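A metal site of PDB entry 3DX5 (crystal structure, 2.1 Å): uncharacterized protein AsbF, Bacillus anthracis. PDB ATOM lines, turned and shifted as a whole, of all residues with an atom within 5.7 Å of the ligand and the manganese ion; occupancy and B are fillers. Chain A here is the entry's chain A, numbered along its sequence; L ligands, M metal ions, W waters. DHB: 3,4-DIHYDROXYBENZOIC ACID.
OH of Tyr 70 sits at hydrogen-bond distance from O1 of the ligand (2.5 Å). OH of Tyr 217 lies within hydrogen-bond range of O1 of the ligand (2.6 Å). An oxygen (O3) of the ligand lies close to the side-chain amino group (NZ) of Lys 200 (2.8 Å). A ring nitrogen (NE2) of His 175 lies within hydrogen-bond range of an oxygen (O4) of the ligand (2.8 Å). An oxygen (O2) of the ligand lies within salt-bridge range of the guanidinium group (NH2) of Arg 102 (2.8 Å). An oxygen (O4) of the ligand sits close to a ring nitrogen (NE2) of His 144 (3.5 Å). O4 of the ligand is in hydrogen-bond range of O of Phe 211, 3.4 Å away.
The side-chain carboxylate (OE1) of Glu 142 is in salt-bridge range of the guanidinium group (NH2) of Arg 102 (2.7 Å). The side-chain carboxylate (OE2) of Glu 142 sits close to a ring nitrogen (NE2) of His 144, at 3.5 Å. The side-chain carboxylate of Glu 142 lies within hydrogen-bond range of the side-chain amide nitrogen of Asn 170, 3.0 Å away. NZ of Lys 200 lies within salt-bridge range of OD1 of Asp 172 (3.1 Å). ND2 of Asn 170 sits at hydrogen-bond distance from NE2 of His 198, at 3.2 Å. OE1 of Glu 253 sits close to NZ of Lys 200 (2.8 Å). The side-chain hydroxyl (OH) of Tyr 70 lies within hydrogen-bond range of the indole nitrogen (NE1) of Trp 35 (2.8 Å). A ring nitrogen (NE2) of His 144 lies within hydrogen-bond range of a ring nitrogen (NE2) of His 175 (3.4 Å).
Ile 8 touches the ligand (CD1 to O1, 3.5 Å). CZ of Phe 104 touches O2 of the ligand, 3.9 Å away. CE2 of Phe 255 touches C4 of the ligand (3.5 Å). Within 4 Å of the ligand: Ile 8, Tyr 70, Arg 102, Phe 104, Glu 142, His 144, Asp 172, His 175, Lys 200, Phe 211, Tyr 217, Glu 253 and Phe 255. The nearest printed residue that does not touch the ligand is Val 216 (4.1 Å).
Residues that only touch the manganese ion: Lys 200 (3.5 Å). The nearest printed residue that does not touch the manganese ion is His 144 (4.2 Å).
The manganese ion is bound by OE2 of Glu 142 (2.1 Å), O3 of the ligand (2.1 Å), OD2 of Asp 172 (2.1 Å), ND1 of His 198 (2.3 Å), OE1 of Glu 253 (2.3 Å) and OE2 of Glu 253 (2.4 Å).
Water W2 lies within hydrogen-bond range of O of Phe 211 (2.9 Å), O4 of the ligand (3.3 Å) and ND1 of His 144 (3.4 Å).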
ATOM      1  N   ILE A   8       9.522  16.980  30.648  1.00  0.00           N
ATOM      2  CA  ILE A   8      10.290  17.172  29.415  1.00  0.00           C
ATOM      3  C   ILE A   8      11.037  15.888  28.947  1.00  0.00           C
ATOM      4  O   ILE A   8      11.271  15.717  27.775  1.00  0.00           O
ATOM      5  CB  ILE A   8      11.284  18.378  29.533  1.00  0.00           C
ATOM      6  CG1 ILE A   8      11.743  18.865  28.137  1.00  0.00           C
ATOM      7  CG2 ILE A   8      12.465  18.070  30.516  1.00  0.00           C
ATOM      8  CD1 ILE A   8      12.549  20.262  28.176  1.00  0.00           C
ATOM      9  N   TRP A  35       6.816  20.547  32.607  1.00  0.00           N
ATOM     10  CA  TRP A  35       7.162  21.442  31.482  1.00  0.00           C
ATOM     11  C   TRP A  35       5.954  22.381  31.214  1.00  0.00           C
ATOM     12  O   TRP A  35       4.803  21.925  31.260  1.00  0.00           O
ATOM     13  CB  TRP A  35       7.396  20.556  30.268  1.00  0.00           C
ATOM     14  CG  TRP A  35       8.254  21.133  29.185  1.00  0.00           C
ATOM     15  CD1 TRP A  35       9.152  22.194  29.254  1.00  0.00           C
ATOM     16  CD2 TRP A  35       8.340  20.624  27.832  1.00  0.00           C
ATOM     17  NE1 TRP A  35       9.768  22.372  28.010  1.00  0.00           N
ATOM     18  CE2 TRP A  35       9.279  21.422  27.139  1.00  0.00           C
ATOM     19  CE3 TRP A  35       7.699  19.554  27.162  1.00  0.00           C
ATOM     20  CZ2 TRP A  35       9.594  21.189  25.783  1.00  0.00           C
ATOM     21  CZ3 TRP A  35       8.011  19.331  25.816  1.00  0.00           C
ATOM     22  CH2 TRP A  35       8.946  20.150  25.142  1.00  0.00           C
ATOM     23  N   SER A  68       8.400  24.604  34.325  1.00  0.00           N
ATOM     24  CA  SER A  68       9.605  25.025  33.634  1.00  0.00           C
ATOM     25  C   SER A  68       9.318  25.509  32.223  1.00  0.00           C
ATOM     26  O   SER A  68       8.831  24.761  31.370  1.00  0.00           O
ATOM     27  CB  SER A  68      10.664  23.915  33.683  1.00  0.00           C
ATOM     28  OG  SER A  68      10.830  23.519  35.034  1.00  0.00           O
ATOM     29  N   TYR A  70       9.919  29.329  29.444  1.00  0.00           N
ATOM     30  CA  TYR A  70      10.861  30.136  28.671  1.00  0.00           C
ATOM     31  C   TYR A  70      10.186  31.483  28.564  1.00  0.00           C
ATOM     32  O   TYR A  70       9.111  31.589  27.983  1.00  0.00           O
ATOM     33  CB  TYR A  70      11.063  29.545  27.235  1.00  0.00           C
ATOM     34  CG  TYR A  70      11.325  28.030  27.229  1.00  0.00           C
ATOM     35  CD1 TYR A  70      12.642  27.533  27.283  1.00  0.00           C
ATOM     36  CD2 TYR A  70      10.247  27.105  27.212  1.00  0.00           C
ATOM     37  CE1 TYR A  70      12.884  26.138  27.312  1.00  0.00           C
ATOM     38  CE2 TYR A  70      10.495  25.737  27.288  1.00  0.00           C
ATOM     39  CZ  TYR A  70      11.804  25.259  27.330  1.00  0.00           C
ATOM     40  OH  TYR A  70      12.031  23.890  27.370  1.00  0.00           O
ATOM     41  N   ARG A 102      10.613  28.271  36.208  1.00  0.00           N
ATOM     42  CA  ARG A 102      11.969  28.265  35.688  1.00  0.00           C
ATOM     43  C   ARG A 102      12.011  29.044  34.372  1.00  0.00           C
ATOM     44  O   ARG A 102      11.165  28.857  33.490  1.00  0.00           O
ATOM     45  CB  ARG A 102      12.396  26.794  35.450  1.00  0.00           C
ATOM     46  CG  ARG A 102      13.865  26.542  34.975  1.00  0.00           C
ATOM     47  CD  ARG A 102      14.206  26.995  33.502  1.00  0.00           C
ATOM     48  NE  ARG A 102      13.322  26.529  32.414  1.00  0.00           N
ATOM     49  CZ  ARG A 102      13.454  25.366  31.793  1.00  0.00           C
ATOM     50  NH1 ARG A 102      12.619  25.045  30.794  1.00  0.00           N
ATOM     51  NH2 ARG A 102      14.427  24.517  32.169  1.00  0.00           N
ATOM     52  N   PHE A 104      15.080  31.175  31.523  1.00  0.00           N
ATOM     53  CA  PHE A 104      16.477  31.368  31.128  1.00  0.00           C
ATOM     54  C   PHE A 104      16.745  32.844  31.014  1.00  0.00           C
ATOM     55  O   PHE A 104      15.837  33.613  30.685  1.00  0.00           O
ATOM     56  CB  PHE A 104      16.763  30.670  29.781  1.00  0.00           C
ATOM     57  CG  PHE A 104      16.677  29.171  29.881  1.00  0.00           C
ATOM     58  CD1 PHE A 104      17.701  28.444  30.485  1.00  0.00           C
ATOM     59  CD2 PHE A 104      15.559  28.489  29.415  1.00  0.00           C
ATOM     60  CE1 PHE A 104      17.628  27.066  30.605  1.00  0.00           C
ATOM     61  CE2 PHE A 104      15.491  27.092  29.516  1.00  0.00           C
ATOM     62  CZ  PHE A 104      16.503  26.394  30.117  1.00  0.00           C
ATOM     63  N   GLU A 142      17.852  29.340  35.342  1.00  0.00           N
ATOM     64  CA  GLU A 142      18.632  28.117  35.222  1.00  0.00           C
ATOM     65  C   GLU A 142      20.070  28.472  34.761  1.00  0.00           C
ATOM     66  O   GLU A 142      20.247  29.305  33.907  1.00  0.00           O
ATOM     67  CB  GLU A 142      17.926  27.161  34.242  1.00  0.00           C
ATOM     68  CG  GLU A 142      18.621  25.821  34.129  1.00  0.00           C
ATOM     69  CD  GLU A 142      17.706  24.758  33.603  1.00  0.00           C
ATOM     70  OE1 GLU A 142      16.496  24.765  33.919  1.00  0.00           O
ATOM     71  OE2 GLU A 142      18.206  23.899  32.870  1.00  0.00           O
ATOM     72  N   HIS A 144      22.976  28.032  32.538  1.00  0.00           N
ATOM     73  CA  HIS A 144      23.002  27.528  31.164  1.00  0.00           C
ATOM     74  C   HIS A 144      24.037  28.226  30.279  1.00  0.00           C
ATOM     75  O   HIS A 144      24.162  29.451  30.371  1.00  0.00           O
ATOM     76  CB  HIS A 144      21.656  27.773  30.507  1.00  0.00           C
ATOM     77  CG  HIS A 144      20.973  26.510  30.121  1.00  0.00           C
ATOM     78  ND1 HIS A 144      20.593  26.233  28.827  1.00  0.00           N
ATOM     79  CD2 HIS A 144      20.693  25.405  30.859  1.00  0.00           C
ATOM     80  CE1 HIS A 144      20.027  25.043  28.806  1.00  0.00           C
ATOM     81  NE2 HIS A 144      20.089  24.516  30.021  1.00  0.00           N
ATOM     82  N   ASN A 170      17.881  27.877  39.642  1.00  0.00           N
ATOM     83  CA  ASN A 170      17.837  26.448  39.410  1.00  0.00           C
ATOM     84  C   ASN A 170      19.254  26.024  39.018  1.00  0.00           C
ATOM     85  O   ASN A 170      19.730  26.350  37.907  1.00  0.00           O
ATOM     86  CB  ASN A 170      16.875  26.079  38.253  1.00  0.00           C
ATOM     87  CG  ASN A 170      16.805  24.565  38.051  1.00  0.00           C
ATOM     88  OD1 ASN A 170      16.994  23.803  38.993  1.00  0.00           O
ATOM     89  ND2 ASN A 170      16.603  24.140  36.830  1.00  0.00           N
ATOM     90  N   ASP A 172      21.991  23.849  37.648  1.00  0.00           N
ATOM     91  CA  ASP A 172      22.138  22.695  36.731  1.00  0.00           C
ATOM     92  C   ASP A 172      23.646  22.386  36.740  1.00  0.00           C
ATOM     93  O   ASP A 172      24.441  23.083  36.097  1.00  0.00           O
ATOM     94  CB  ASP A 172      21.580  23.083  35.353  1.00  0.00           C
ATOM     95  CG  ASP A 172      21.568  21.927  34.358  1.00  0.00           C
ATOM     96  OD1 ASP A 172      22.522  21.121  34.312  1.00  0.00           O
ATOM     97  OD2 ASP A 172      20.610  21.861  33.571  1.00  0.00           O
ATOM     98  N   HIS A 175      25.895  21.987  33.527  1.00  0.00           N
ATOM     99  CA  HIS A 175      26.235  23.209  32.858  1.00  0.00           C
ATOM    100  C   HIS A 175      27.213  24.061  33.629  1.00  0.00           C
ATOM    101  O   HIS A 175      28.008  24.779  33.036  1.00  0.00           O
ATOM    102  CB  HIS A 175      24.974  24.002  32.469  1.00  0.00           C
ATOM    103  CG  HIS A 175      24.172  23.293  31.426  1.00  0.00           C
ATOM    104  ND1 HIS A 175      24.731  22.841  30.253  1.00  0.00           N
ATOM    105  CD2 HIS A 175      22.880  22.884  31.420  1.00  0.00           C
ATOM    106  CE1 HIS A 175      23.793  22.229  29.542  1.00  0.00           C
ATOM    107  NE2 HIS A 175      22.665  22.246  30.220  1.00  0.00           N
ATOM    108  N   HIS A 198      18.998  20.630  38.841  1.00  0.00           N
ATOM    109  CA  HIS A 198      18.935  19.673  37.721  1.00  0.00           C
ATOM    110  C   HIS A 198      20.165  18.816  37.806  1.00  0.00           C
ATOM    111  O   HIS A 198      21.275  19.341  37.926  1.00  0.00           O
ATOM    112  CB  HIS A 198      18.926  20.416  36.367  1.00  0.00           C
ATOM    113  CG  HIS A 198      17.569  20.885  35.949  1.00  0.00           C
ATOM    114  ND1 HIS A 198      17.328  21.514  34.740  1.00  0.00           N
ATOM    115  CD2 HIS A 198      16.369  20.800  36.582  1.00  0.00           C
ATOM    116  CE1 HIS A 198      16.028  21.777  34.634  1.00  0.00           C
ATOM    117  NE2 HIS A 198      15.427  21.356  35.741  1.00  0.00           N
ATOM    118  N   LYS A 200      22.170  15.995  35.571  1.00  0.00           N
ATOM    119  CA  LYS A 200      22.353  15.130  34.395  1.00  0.00           C
ATOM    120  C   LYS A 200      23.860  15.000  34.196  1.00  0.00           C
ATOM    121  O   LYS A 200      24.632  15.745  34.811  1.00  0.00           O
ATOM    122  CB  LYS A 200      21.617  15.687  33.139  1.00  0.00           C
ATOM    123  CG  LYS A 200      22.018  17.128  32.681  1.00  0.00           C
ATOM    124  CD  LYS A 200      21.282  17.487  31.371  1.00  0.00           C
ATOM    125  CE  LYS A 200      21.682  18.883  30.825  1.00  0.00           C
ATOM    126  NZ  LYS A 200      21.281  19.993  31.757  1.00  0.00           N
ATOM    127  N   PHE A 211      23.587  18.712  24.405  1.00  0.00           N
ATOM    128  CA  PHE A 211      22.654  19.500  25.198  1.00  0.00           C
ATOM    129  C   PHE A 211      22.214  20.826  24.602  1.00  0.00           C
ATOM    130  O   PHE A 211      21.426  21.536  25.222  1.00  0.00           O
ATOM    131  CB  PHE A 211      23.164  19.705  26.611  1.00  0.00           C
ATOM    132  CG  PHE A 211      23.346  18.423  27.357  1.00  0.00           C
ATOM    133  CD1 PHE A 211      22.300  17.488  27.451  1.00  0.00           C
ATOM    134  CD2 PHE A 211      24.569  18.128  27.932  1.00  0.00           C
ATOM    135  CE1 PHE A 211      22.477  16.281  28.149  1.00  0.00           C
ATOM    136  CE2 PHE A 211      24.743  16.932  28.639  1.00  0.00           C
ATOM    137  CZ  PHE A 211      23.702  16.013  28.739  1.00  0.00           C
ATOM    138  N   GLU A 212      22.691  21.169  23.421  1.00  0.00           N
ATOM    139  CA  GLU A 212      22.175  22.374  22.818  1.00  0.00           C
ATOM    140  C   GLU A 212      20.653  22.209  22.616  1.00  0.00           C
ATOM    141  O   GLU A 212      20.205  21.157  22.151  1.00  0.00           O
ATOM    142  CB  GLU A 212      22.869  22.645  21.476  1.00  0.00           C
ATOM    143  CG  GLU A 212      24.332  23.093  21.679  1.00  0.00           C
ATOM    144  CD  GLU A 212      25.102  23.205  20.365  1.00  0.00           C
ATOM    145  OE1 GLU A 212      24.434  23.155  19.301  1.00  0.00           O
ATOM    146  OE2 GLU A 212      26.353  23.328  20.389  1.00  0.00           O
ATOM    147  N   PRO A 213      19.867  23.245  22.971  1.00  0.00           N
ATOM    148  CA  PRO A 213      18.403  23.158  22.970  1.00  0.00           C
ATOM    149  C   PRO A 213      17.846  22.634  21.640  1.00  0.00           C
ATOM    150  O   PRO A 213      16.997  21.756  21.641  1.00  0.00           O
ATOM    151  CB  PRO A 213      17.948  24.602  23.293  1.00  0.00           C
ATOM    152  CG  PRO A 213      19.053  25.056  24.282  1.00  0.00           C
ATOM    153  CD  PRO A 213      20.349  24.509  23.616  1.00  0.00           C
ATOM    154  N   VAL A 216      18.321  18.923  21.621  1.00  0.00           N
ATOM    155  CA  VAL A 216      17.445  18.337  22.636  1.00  0.00           C
ATOM    156  C   VAL A 216      15.988  18.268  22.153  1.00  0.00           C
ATOM    157  O   VAL A 216      15.324  17.228  22.337  1.00  0.00           O
ATOM    158  CB  VAL A 216      17.556  19.060  23.991  1.00  0.00           C
ATOM    159  CG1 VAL A 216      16.386  18.631  24.968  1.00  0.00           C
ATOM    160  CG2 VAL A 216      18.912  18.772  24.654  1.00  0.00           C
ATOM    161  N   TYR A 217      15.486  19.346  21.519  1.00  0.00           N
ATOM    162  CA  TYR A 217      14.063  19.384  21.141  1.00  0.00           C
ATOM    163  C   TYR A 217      13.716  18.560  19.896  1.00  0.00           C
ATOM    164  O   TYR A 217      12.556  18.163  19.745  1.00  0.00           O
ATOM    165  CB  TYR A 217      13.517  20.824  20.949  1.00  0.00           C
ATOM    166  CG  TYR A 217      13.849  21.744  22.112  1.00  0.00           C
ATOM    167  CD1 TYR A 217      13.836  21.289  23.440  1.00  0.00           C
ATOM    168  CD2 TYR A 217      14.155  23.095  21.869  1.00  0.00           C
ATOM    169  CE1 TYR A 217      14.165  22.151  24.518  1.00  0.00           C
ATOM    170  CE2 TYR A 217      14.454  23.961  22.925  1.00  0.00           C
ATOM    171  CZ  TYR A 217      14.482  23.489  24.230  1.00  0.00           C
ATOM    172  OH  TYR A 217      14.800  24.399  25.235  1.00  0.00           O
ATOM    173  N   GLU A 253      17.199  15.178  35.108  1.00  0.00           N
ATOM    174  CA  GLU A 253      16.889  15.774  33.812  1.00  0.00           C
ATOM    175  C   GLU A 253      17.429  14.926  32.685  1.00  0.00           C
ATOM    176  O   GLU A 253      18.465  15.262  32.072  1.00  0.00           O
ATOM    177  CB  GLU A 253      17.512  17.167  33.728  1.00  0.00           C
ATOM    178  CG  GLU A 253      16.916  18.035  32.607  1.00  0.00           C
ATOM    179  CD  GLU A 253      17.559  19.415  32.540  1.00  0.00           C
ATOM    180  OE1 GLU A 253      18.761  19.514  32.877  1.00  0.00           O
ATOM    181  OE2 GLU A 253      16.863  20.389  32.154  1.00  0.00           O
ATOM    182  N   PHE A 255      17.451  13.568  28.960  1.00  0.00           N
ATOM    183  CA  PHE A 255      17.031  13.957  27.625  1.00  0.00           C
ATOM    184  C   PHE A 255      17.229  12.799  26.622  1.00  0.00           C
ATOM    185  O   PHE A 255      16.973  12.960  25.440  1.00  0.00           O
ATOM    186  CB  PHE A 255      17.836  15.164  27.167  1.00  0.00           C
ATOM    187  CG  PHE A 255      17.481  16.439  27.876  1.00  0.00           C
ATOM    188  CD1 PHE A 255      16.134  16.810  28.029  1.00  0.00           C
ATOM    189  CD2 PHE A 255      18.472  17.287  28.355  1.00  0.00           C
ATOM    190  CE1 PHE A 255      15.782  17.984  28.606  1.00  0.00           C
ATOM    191  CE2 PHE A 255      18.122  18.499  28.965  1.00  0.00           C
ATOM    192  CZ  PHE A 255      16.774  18.843  29.104  1.00  0.00           C
HETATM  193  C1  DHB L   1      16.574  22.562  28.501  1.00  0.00           C
HETATM  194  C2  DHB L   1      17.253  22.407  29.708  1.00  0.00           C
HETATM  195  C3  DHB L   1      18.597  22.008  29.727  1.00  0.00           C
HETATM  196  O3  DHB L   1      19.327  21.834  30.874  1.00  0.00           O
HETATM  197  C4  DHB L   1      19.269  21.791  28.442  1.00  0.00           C
HETATM  198  O4  DHB L   1      20.562  21.414  28.500  1.00  0.00           O
HETATM  199  C5  DHB L   1      18.583  21.977  27.242  1.00  0.00           C
HETATM  200  C6  DHB L   1      17.239  22.357  27.293  1.00  0.00           C
HETATM  201  C   DHB L   1      15.112  22.979  28.525  1.00  0.00           C
HETATM  202  O1  DHB L   1      14.451  23.184  27.509  1.00  0.00           O
HETATM  203  O2  DHB L   1      14.492  23.120  29.696  1.00  0.00           O
HETATM  204 MN    MN M   1      18.588  21.856  32.873  1.00  0.00          MN
HETATM  205  O   HOH W   1      14.380  20.969  31.573  1.00  0.00           O
HETATM  206  O   HOH W   2      22.113  23.865  26.871  1.00  0.00           O
